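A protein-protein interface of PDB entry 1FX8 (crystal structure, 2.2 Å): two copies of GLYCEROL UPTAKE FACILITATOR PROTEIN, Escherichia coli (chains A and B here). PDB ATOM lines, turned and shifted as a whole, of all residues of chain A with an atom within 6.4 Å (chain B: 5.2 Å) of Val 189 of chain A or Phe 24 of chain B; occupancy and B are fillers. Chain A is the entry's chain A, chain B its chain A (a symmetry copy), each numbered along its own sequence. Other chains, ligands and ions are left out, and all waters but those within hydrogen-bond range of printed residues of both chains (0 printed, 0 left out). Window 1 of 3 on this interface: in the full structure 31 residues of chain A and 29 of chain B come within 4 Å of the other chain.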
ATOM      1  N   TRP A  42       8.839 -18.719  13.043  1.00  0.00           N
ATOM      2  CA  TRP A  42       8.117 -18.180  11.896  1.00  0.00           C
ATOM      3  C   TRP A  42       6.701 -17.711  12.256  1.00  0.00           C
ATOM      4  O   TRP A  42       6.272 -16.636  11.841  1.00  0.00           O
ATOM      5  CB  TRP A  42       8.043 -19.224  10.770  1.00  0.00           C
ATOM      6  CG  TRP A  42       7.036 -18.879   9.705  1.00  0.00           C
ATOM      7  CD1 TRP A  42       5.860 -19.531   9.450  1.00  0.00           C
ATOM      8  CD2 TRP A  42       7.070 -17.751   8.816  1.00  0.00           C
ATOM      9  NE1 TRP A  42       5.162 -18.876   8.463  1.00  0.00           N
ATOM     10  CE2 TRP A  42       5.878 -17.781   8.058  1.00  0.00           C
ATOM     11  CE3 TRP A  42       7.990 -16.715   8.591  1.00  0.00           C
ATOM     12  CZ2 TRP A  42       5.578 -16.813   7.086  1.00  0.00           C
ATOM     13  CZ3 TRP A  42       7.689 -15.748   7.622  1.00  0.00           C
ATOM     14  CH2 TRP A  42       6.491 -15.808   6.885  1.00  0.00           C
ATOM     15  N   SER A  45       6.809 -14.590  14.237  1.00  0.00           N
ATOM     16  CA  SER A  45       7.208 -13.505  13.363  1.00  0.00           C
ATOM     17  C   SER A  45       6.098 -13.049  12.416  1.00  0.00           C
ATOM     18  O   SER A  45       5.896 -11.851  12.232  1.00  0.00           O
ATOM     19  CB  SER A  45       8.456 -13.912  12.572  1.00  0.00           C
ATOM     20  OG  SER A  45       9.529 -14.164  13.469  1.00  0.00           O
ATOM     21  N   ILE A 158      17.418  -2.013   7.562  1.00  0.00           N
ATOM     22  CA  ILE A 158      16.747  -2.791   6.532  1.00  0.00           C
ATOM     23  C   ILE A 158      15.253  -2.464   6.556  1.00  0.00           C
ATOM     24  O   ILE A 158      14.633  -2.286   5.509  1.00  0.00           O
ATOM     25  CB  ILE A 158      16.952  -4.305   6.770  1.00  0.00           C
ATOM     26  CG1 ILE A 158      18.395  -4.685   6.429  1.00  0.00           C
ATOM     27  CG2 ILE A 158      15.962  -5.112   5.946  1.00  0.00           C
ATOM     28  CD1 ILE A 158      18.712  -6.153   6.614  1.00  0.00           C
ATOM     29  N   LEU A 162      13.472  -0.685   3.374  1.00  0.00           N
ATOM     30  CA  LEU A 162      12.449  -1.406   2.622  1.00  0.00           C
ATOM     31  C   LEU A 162      11.075  -0.766   2.754  1.00  0.00           C
ATOM     32  O   LEU A 162      10.232  -0.911   1.868  1.00  0.00           O
ATOM     33  CB  LEU A 162      12.397  -2.879   3.043  1.00  0.00           C
ATOM     34  CG  LEU A 162      13.335  -3.820   2.275  1.00  0.00           C
ATOM     35  CD1 LEU A 162      12.891  -3.913   0.818  1.00  0.00           C
ATOM     36  CD2 LEU A 162      14.764  -3.325   2.366  1.00  0.00           C
ATOM     37  N   GLY A 184       4.272  -5.809   6.549  1.00  0.00           N
ATOM     38  CA  GLY A 184       4.059  -6.803   7.579  1.00  0.00           C
ATOM     39  C   GLY A 184       4.900  -8.039   7.290  1.00  0.00           C
ATOM     40  O   GLY A 184       5.529  -8.592   8.190  1.00  0.00           O
ATOM     41  N   LEU A 185       4.915  -8.470   6.030  1.00  0.00           N
ATOM     42  CA  LEU A 185       5.692  -9.641   5.631  1.00  0.00           C
ATOM     43  C   LEU A 185       7.186  -9.359   5.758  1.00  0.00           C
ATOM     44  O   LEU A 185       7.980 -10.272   5.994  1.00  0.00           O
ATOM     45  CB  LEU A 185       5.352 -10.056   4.192  1.00  0.00           C
ATOM     46  CG  LEU A 185       3.932 -10.587   3.963  1.00  0.00           C
ATOM     47  CD1 LEU A 185       3.771 -11.002   2.500  1.00  0.00           C
ATOM     48  CD2 LEU A 185       3.653 -11.777   4.890  1.00  0.00           C
ATOM     49  N   LEU A 186       7.564  -8.093   5.605  1.00  0.00           N
ATOM     50  CA  LEU A 186       8.960  -7.703   5.727  1.00  0.00           C
ATOM     51  C   LEU A 186       9.398  -7.938   7.173  1.00  0.00           C
ATOM     52  O   LEU A 186      10.468  -8.488   7.431  1.00  0.00           O
ATOM     53  CB  LEU A 186       9.134  -6.226   5.364  1.00  0.00           C
ATOM     54  CG  LEU A 186      10.488  -5.619   5.745  1.00  0.00           C
ATOM     55  CD1 LEU A 186      11.604  -6.275   4.943  1.00  0.00           C
ATOM     56  CD2 LEU A 186      10.451  -4.115   5.498  1.00  0.00           C
ATOM     57  N   ILE A 187       8.554  -7.512   8.109  1.00  0.00           N
ATOM     58  CA  ILE A 187       8.817  -7.681   9.531  1.00  0.00           C
ATOM     59  C   ILE A 187       8.866  -9.172   9.855  1.00  0.00           C
ATOM     60  O   ILE A 187       9.673  -9.614  10.678  1.00  0.00           O
ATOM     61  CB  ILE A 187       7.719  -6.977  10.364  1.00  0.00           C
ATOM     62  CG1 ILE A 187       7.915  -5.461  10.266  1.00  0.00           C
ATOM     63  CG2 ILE A 187       7.765  -7.427  11.816  1.00  0.00           C
ATOM     64  CD1 ILE A 187       6.726  -4.656  10.716  1.00  0.00           C
ATOM     65  N   ALA A 188       8.015  -9.947   9.192  1.00  0.00           N
ATOM     66  CA  ALA A 188       7.983 -11.381   9.400  1.00  0.00           C
ATOM     67  C   ALA A 188       9.318 -12.036   9.010  1.00  0.00           C
ATOM     68  O   ALA A 188       9.845 -12.849   9.763  1.00  0.00           O
ATOM     69  CB  ALA A 188       6.845 -11.998   8.602  1.00  0.00           C
ATOM     70  N   VAL A 189       9.870 -11.685   7.848  1.00  0.00           N
ATOM     71  CA  VAL A 189      11.139 -12.289   7.438  1.00  0.00           C
ATOM     72  C   VAL A 189      12.319 -11.792   8.280  1.00  0.00           C
ATOM     73  O   VAL A 189      13.290 -12.522   8.470  1.00  0.00           O
ATOM     74  CB  VAL A 189      11.432 -12.089   5.911  1.00  0.00           C
ATOM     75  CG1 VAL A 189      10.309 -12.694   5.094  1.00  0.00           C
ATOM     76  CG2 VAL A 189      11.586 -10.628   5.575  1.00  0.00           C
ATOM     77  N   ILE A 190      12.244 -10.562   8.789  1.00  0.00           N
ATOM     78  CA  ILE A 190      13.313 -10.054   9.650  1.00  0.00           C
ATOM     79  C   ILE A 190      13.254 -10.847  10.969  1.00  0.00           C
ATOM     80  O   ILE A 190      14.275 -11.289  11.487  1.00  0.00           O
ATOM     81  CB  ILE A 190      13.136  -8.540   9.968  1.00  0.00           C
ATOM     82  CG1 ILE A 190      13.462  -7.693   8.729  1.00  0.00           C
ATOM     83  CG2 ILE A 190      14.050  -8.134  11.121  1.00  0.00           C
ATOM     84  CD1 ILE A 190      13.115  -6.227   8.881  1.00  0.00           C
ATOM     85  N   GLY A 191      12.044 -11.033  11.494  1.00  0.00           N
ATOM     86  CA  GLY A 191      11.882 -11.762  12.736  1.00  0.00           C
ATOM     87  C   GLY A 191      12.305 -13.214  12.646  1.00  0.00           C
ATOM     88  O   GLY A 191      12.838 -13.773  13.602  1.00  0.00           O
ATOM     89  N   ALA A 192      12.071 -13.831  11.494  1.00  0.00           N
ATOM     90  CA  ALA A 192      12.431 -15.227  11.294  1.00  0.00           C
ATOM     91  C   ALA A 192      13.930 -15.425  11.099  1.00  0.00           C
ATOM     92  O   ALA A 192      14.497 -16.410  11.566  1.00  0.00           O
ATOM     93  CB  ALA A 192      11.684 -15.781  10.100  1.00  0.00           C
ATOM     94  N   SER A 193      14.574 -14.483  10.418  1.00  0.00           N
ATOM     95  CA  SER A 193      16.002 -14.601  10.145  1.00  0.00           C
ATOM     96  C   SER A 193      16.936 -14.020  11.203  1.00  0.00           C
ATOM     97  O   SER A 193      18.063 -14.487  11.356  1.00  0.00           O
ATOM     98  CB  SER A 193      16.326 -13.970   8.787  1.00  0.00           C
ATOM     99  OG  SER A 193      15.960 -12.601   8.754  1.00  0.00           O
ATOM    100  N   MET A 194      16.466 -13.019  11.943  1.00  0.00           N
ATOM    101  CA  MET A 194      17.293 -12.364  12.953  1.00  0.00           C
ATOM    102  C   MET A 194      16.691 -12.330  14.350  1.00  0.00           C
ATOM    103  O   MET A 194      17.381 -11.996  15.318  1.00  0.00           O
ATOM    104  CB  MET A 194      17.585 -10.926  12.518  1.00  0.00           C
ATOM    105  CG  MET A 194      18.493 -10.790  11.310  1.00  0.00           C
ATOM    106  SD  MET A 194      20.189 -11.321  11.628  1.00  0.00           S
ATOM    107  CE  MET A 194      20.497 -12.368  10.176  1.00  0.00           C
ATOM    108  N   GLY A 195      15.405 -12.662  14.448  1.00  0.00           N
ATOM    109  CA  GLY A 195      14.711 -12.643  15.721  1.00  0.00           C
ATOM    110  C   GLY A 195      15.358 -13.416  16.859  1.00  0.00           C
ATOM    111  O   GLY A 195      15.336 -12.952  17.998  1.00  0.00           O
ATOM    112  N   GLY B  19      22.279  -9.504  -2.024  1.00  0.00           N
ATOM    113  CA  GLY B  19      22.752  -9.564  -0.654  1.00  0.00           C
ATOM    114  C   GLY B  19      21.579  -9.643   0.307  1.00  0.00           C
ATOM    115  O   GLY B  19      21.629 -10.354   1.311  1.00  0.00           O
ATOM    116  N   LEU B  20      20.513  -8.915  -0.014  1.00  0.00           N
ATOM    117  CA  LEU B  20      19.313  -8.895   0.820  1.00  0.00           C
ATOM    118  C   LEU B  20      18.677 -10.281   0.937  1.00  0.00           C
ATOM    119  O   LEU B  20      18.360 -10.724   2.043  1.00  0.00           O
ATOM    120  CB  LEU B  20      18.286  -7.915   0.247  1.00  0.00           C
ATOM    121  CG  LEU B  20      17.396  -7.104   1.198  1.00  0.00           C
ATOM    122  CD1 LEU B  20      15.949  -7.326   0.821  1.00  0.00           C
ATOM    123  CD2 LEU B  20      17.636  -7.484   2.648  1.00  0.00           C
ATOM    124  N   LEU B  21      18.485 -10.977  -0.183  1.00  0.00           N
ATOM    125  CA  LEU B  21      17.868 -12.289  -0.076  1.00  0.00           C
ATOM    126  C   LEU B  21      18.775 -13.321   0.598  1.00  0.00           C
ATOM    127  O   LEU B  21      18.282 -14.264   1.213  1.00  0.00           O
ATOM    128  CB  LEU B  21      17.331 -12.793  -1.434  1.00  0.00           C
ATOM    129  CG  LEU B  21      18.014 -13.319  -2.707  1.00  0.00           C
ATOM    130  CD1 LEU B  21      18.513 -12.183  -3.557  1.00  0.00           C
ATOM    131  CD2 LEU B  21      19.095 -14.305  -2.361  1.00  0.00           C
ATOM    132  N   ILE B  22      20.090 -13.136   0.515  1.00  0.00           N
ATOM    133  CA  ILE B  22      21.001 -14.066   1.177  1.00  0.00           C
ATOM    134  C   ILE B  22      20.950 -13.784   2.679  1.00  0.00           C
ATOM    135  O   ILE B  22      21.013 -14.708   3.492  1.00  0.00           O
ATOM    136  CB  ILE B  22      22.471 -13.928   0.666  1.00  0.00           C
ATOM    137  CG1 ILE B  22      22.752 -14.975  -0.410  1.00  0.00           C
ATOM    138  CG2 ILE B  22      23.463 -14.171   1.795  1.00  0.00           C
ATOM    139  CD1 ILE B  22      22.008 -14.765  -1.671  1.00  0.00           C
ATOM    140  N   PHE B  23      20.823 -12.507   3.033  1.00  0.00           N
ATOM    141  CA  PHE B  23      20.753 -12.081   4.430  1.00  0.00           C
ATOM    142  C   PHE B  23      19.573 -12.763   5.118  1.00  0.00           C
ATOM    143  O   PHE B  23      19.731 -13.386   6.161  1.00  0.00           O
ATOM    144  CB  PHE B  23      20.595 -10.555   4.517  1.00  0.00           C
ATOM    145  CG  PHE B  23      20.557 -10.030   5.927  1.00  0.00           C
ATOM    146  CD1 PHE B  23      21.731  -9.844   6.649  1.00  0.00           C
ATOM    147  CD2 PHE B  23      19.342  -9.747   6.546  1.00  0.00           C
ATOM    148  CE1 PHE B  23      21.694  -9.382   7.969  1.00  0.00           C
ATOM    149  CE2 PHE B  23      19.296  -9.285   7.865  1.00  0.00           C
ATOM    150  CZ  PHE B  23      20.472  -9.103   8.573  1.00  0.00           C
ATOM    151  N   PHE B  24      18.392 -12.639   4.521  1.00  0.00           N
ATOM    152  CA  PHE B  24      17.181 -13.252   5.062  1.00  0.00           C
ATOM    153  C   PHE B  24      17.291 -14.772   4.983  1.00  0.00           C
ATOM    154  O   PHE B  24      16.981 -15.480   5.942  1.00  0.00           O
ATOM    155  CB  PHE B  24      15.948 -12.812   4.261  1.00  0.00           C
ATOM    156  CG  PHE B  24      15.571 -11.365   4.447  1.00  0.00           C
ATOM    157  CD1 PHE B  24      15.146 -10.602   3.359  1.00  0.00           C
ATOM    158  CD2 PHE B  24      15.594 -10.777   5.709  1.00  0.00           C
ATOM    159  CE1 PHE B  24      14.743  -9.258   3.520  1.00  0.00           C
ATOM    160  CE2 PHE B  24      15.196  -9.441   5.887  1.00  0.00           C
ATOM    161  CZ  PHE B  24      14.768  -8.680   4.784  1.00  0.00           C
ATOM    162  N   GLY B  25      17.728 -15.265   3.828  1.00  0.00           N
ATOM    163  CA  GLY B  25      17.853 -16.699   3.627  1.00  0.00           C
ATOM    164  C   GLY B  25      18.849 -17.396   4.535  1.00  0.00           C
ATOM    165  O   GLY B  25      18.492 -18.316   5.263  1.00  0.00           O
ATOM    166  N   VAL B  26      20.108 -16.976   4.476  1.00  0.00           N
ATOM    167  CA  VAL B  26      21.153 -17.565   5.302  1.00  0.00           C
ATOM    168  C   VAL B  26      20.843 -17.273   6.771  1.00  0.00           C
ATOM    169  O   VAL B  26      21.147 -18.077   7.662  1.00  0.00           O
ATOM    170  CB  VAL B  26      22.546 -16.992   4.909  1.00  0.00           C
ATOM    171  CG1 VAL B  26      23.636 -17.516   5.849  1.00  0.00           C
ATOM    172  CG2 VAL B  26      22.867 -17.384   3.468  1.00  0.00           C
ATOM    173  N   GLY B  27      20.210 -16.125   7.017  1.00  0.00           N
ATOM    174  CA  GLY B  27      19.850 -15.767   8.374  1.00  0.00           C
ATOM    175  C   GLY B  27      18.907 -16.773   9.028  1.00  0.00           C
ATOM    176  O   GLY B  27      19.151 -17.215  10.156  1.00  0.00           O
ATOM    177  N   CYS B  28      17.833 -17.153   8.334  1.00  0.00           N
ATOM    178  CA  CYS B  28      16.878 -18.097   8.910  1.00  0.00           C
ATOM    179  C   CYS B  28      17.468 -19.498   9.057  1.00  0.00           C
ATOM    180  O   CYS B  28      17.121 -20.229   9.989  1.00  0.00           O
ATOM    181  CB  CYS B  28      15.566 -18.138   8.095  1.00  0.00           C
ATOM    182  SG  CYS B  28      15.570 -19.025   6.494  1.00  0.00           S
ATOM    183  N   VAL B  29      18.366 -19.879   8.153  1.00  0.00           N
ATOM    184  CA  VAL B  29      18.966 -21.201   8.269  1.00  0.00           C
ATOM    185  C   VAL B  29      19.943 -21.215   9.446  1.00  0.00           C
ATOM    186  O   VAL B  29      20.118 -22.238  10.093  1.00  0.00           O
ATOM    187  CB  VAL B  29      19.699 -21.623   6.979  1.00  0.00           C
ATOM    188  CG1 VAL B  29      20.309 -23.014   7.155  1.00  0.00           C
ATOM    189  CG2 VAL B  29      18.719 -21.636   5.813  1.00  0.00           C
ATOM    190  N   ILE B  47      10.229 -18.351   3.975  1.00  0.00           N
ATOM    191  CA  ILE B  47      11.070 -17.234   4.378  1.00  0.00           C
ATOM    192  C   ILE B  47      12.016 -16.870   3.223  1.00  0.00           C
ATOM    193  O   ILE B  47      12.199 -15.694   2.906  1.00  0.00           O
ATOM    194  CB  ILE B  47      11.906 -17.576   5.631  1.00  0.00           C
ATOM    195  CG1 ILE B  47      10.976 -17.801   6.826  1.00  0.00           C
ATOM    196  CG2 ILE B  47      12.889 -16.436   5.931  1.00  0.00           C
ATOM    197  CD1 ILE B  47      11.640 -18.500   7.996  1.00  0.00           C
ATOM    198  N   LEU B  50       9.818 -15.143   0.448  1.00  0.00           N
ATOM    199  CA  LEU B  50       9.404 -13.789   0.788  1.00  0.00           C
ATOM    200  C   LEU B  50      10.619 -12.878   0.837  1.00  0.00           C
ATOM    201  O   LEU B  50      10.530 -11.695   0.511  1.00  0.00           O
ATOM    202  CB  LEU B  50       8.669 -13.774   2.131  1.00  0.00           C
ATOM    203  CG  LEU B  50       7.297 -14.453   2.078  1.00  0.00           C
ATOM    204  CD1 LEU B  50       6.697 -14.558   3.468  1.00  0.00           C
ATOM    205  CD2 LEU B  50       6.384 -13.658   1.154  1.00  0.00           C
ATOM    206  N   GLY B  51      11.753 -13.434   1.250  1.00  0.00           N
ATOM    207  CA  GLY B  51      12.976 -12.659   1.287  1.00  0.00           C
ATOM    208  C   GLY B  51      13.319 -12.236  -0.133  1.00  0.00           C
ATOM    209  O   GLY B  51      13.718 -11.093  -0.377  1.00  0.00           O
ATOM    210  N   MET B  54      10.996  -9.355  -1.403  1.00  0.00           N
ATOM    211  CA  MET B  54      11.413  -8.045  -0.908  1.00  0.00           C
ATOM    212  C   MET B  54      12.604  -7.506  -1.698  1.00  0.00           C
ATOM    213  O   MET B  54      12.662  -6.319  -2.011  1.00  0.00           O
ATOM    214  CB  MET B  54      11.795  -8.131   0.572  1.00  0.00           C
ATOM    215  CG  MET B  54      10.660  -8.541   1.491  1.00  0.00           C
ATOM    216  SD  MET B  54       9.288  -7.354   1.503  1.00  0.00           S
ATOM    217  CE  MET B  54       7.871  -8.452   1.374  1.00  0.00           C
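The backbone carbonyl oxygen (O) of Gly 27 of chain B lies close to the backbone carbonyl oxygen (O) of Ser 193 of chain A (3.2 Å).
The side-chain hydroxyl (OG) of Ser 45 of chain A lies within hydrogen-bond range of the backbone NH (N) of Ala 192 of chain A. The backbone carbonyl oxygen (O) of Val 189 of chain A lies within hydrogen-bond range of the side-chain hydroxyl (OG) of Ser 193 of chain A (2.7 Å). The side-chain hydroxyl (OG) of Ser 193 of chain A sits at hydrogen-bond distance from the backbone carbonyl oxygen (O) of Ile 190 of chain A. The backbone carbonyl oxygen of Ile 190 of chain A is in hydrogen-bond range of the backbone NH of Gly 195 of chain A (3.5 Å). SG of Cys 28 of chain B sits at hydrogen-bond distance from O of Gly 25 of chain B, 3.2 Å away.
Among the printed residues, merely in contact across the chains: Ser 193 of chain A with Phe 24 of chain B, Ile 158 of chain A with Phe 23 of chain B, Ala 192 of chain A with Ile 47 of chain B, Ser 193 of chain A with Cys 28 of chain B, Val 189 of chain A with Leu 50 of chain B, Trp 42 of chain A with Ile 47 of chain B, Met 194 of chain A with Phe 23 of chain B, Trp 42 of chain A with Leu 50 of chain B, Leu 162 of chain A with Met 54 of chain B, Ile 190 of chain A with Phe 24 of chain B, Val 189 of chain A with Phe 24 of chain B, Met 194 of chain A with Gly 27 of chain B, Ile 158 of chain A with Phe 24 of chain B, Ala 192 of chain A with Cys 28 of chain B, Leu 185 of chain A with Leu 50 of chain B and Leu 186 of chain A with Phe 24 of chain B.
Val 189 of chain A touches two residues of chain B. Of chain A, only Ile 158 (3.9 Å), Leu 186 (3.98 Å), Val 189 (3.8 Å), Ile 190 (3.8 Å) and Ser 193 (3.3 Å) come within 4 Å of Phe 24 of chain B. Of the printed residues of chain A, Phe 23 of chain B touches Ile 158 and Met 194. Of the printed residues of chain B, Leu 186 of chain A touches Phe 24. The nearest printed residue of chain B that does not touch Val 189 of chain A is Ile 47 of chain B (4.2 Å).
Hydrophobic or aromatic side chains of chain A within 4 Å of the printed part of chain B: Trp 42, Ile 158, Leu 162, Leu 185, Leu 186, Val 189, Ile 190, Ala 192 and Met 194. Of the 15 printed residues of chain B, 7 touch a printed residue of chain A. Among the printed residues, 17 pairs touch across the chains. Among the printed residues, no Asp or Glu carboxylate lies within 4 Å of a Lys or Arg side-chain nitrogen of the other chain.
No position is printed for both chains.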
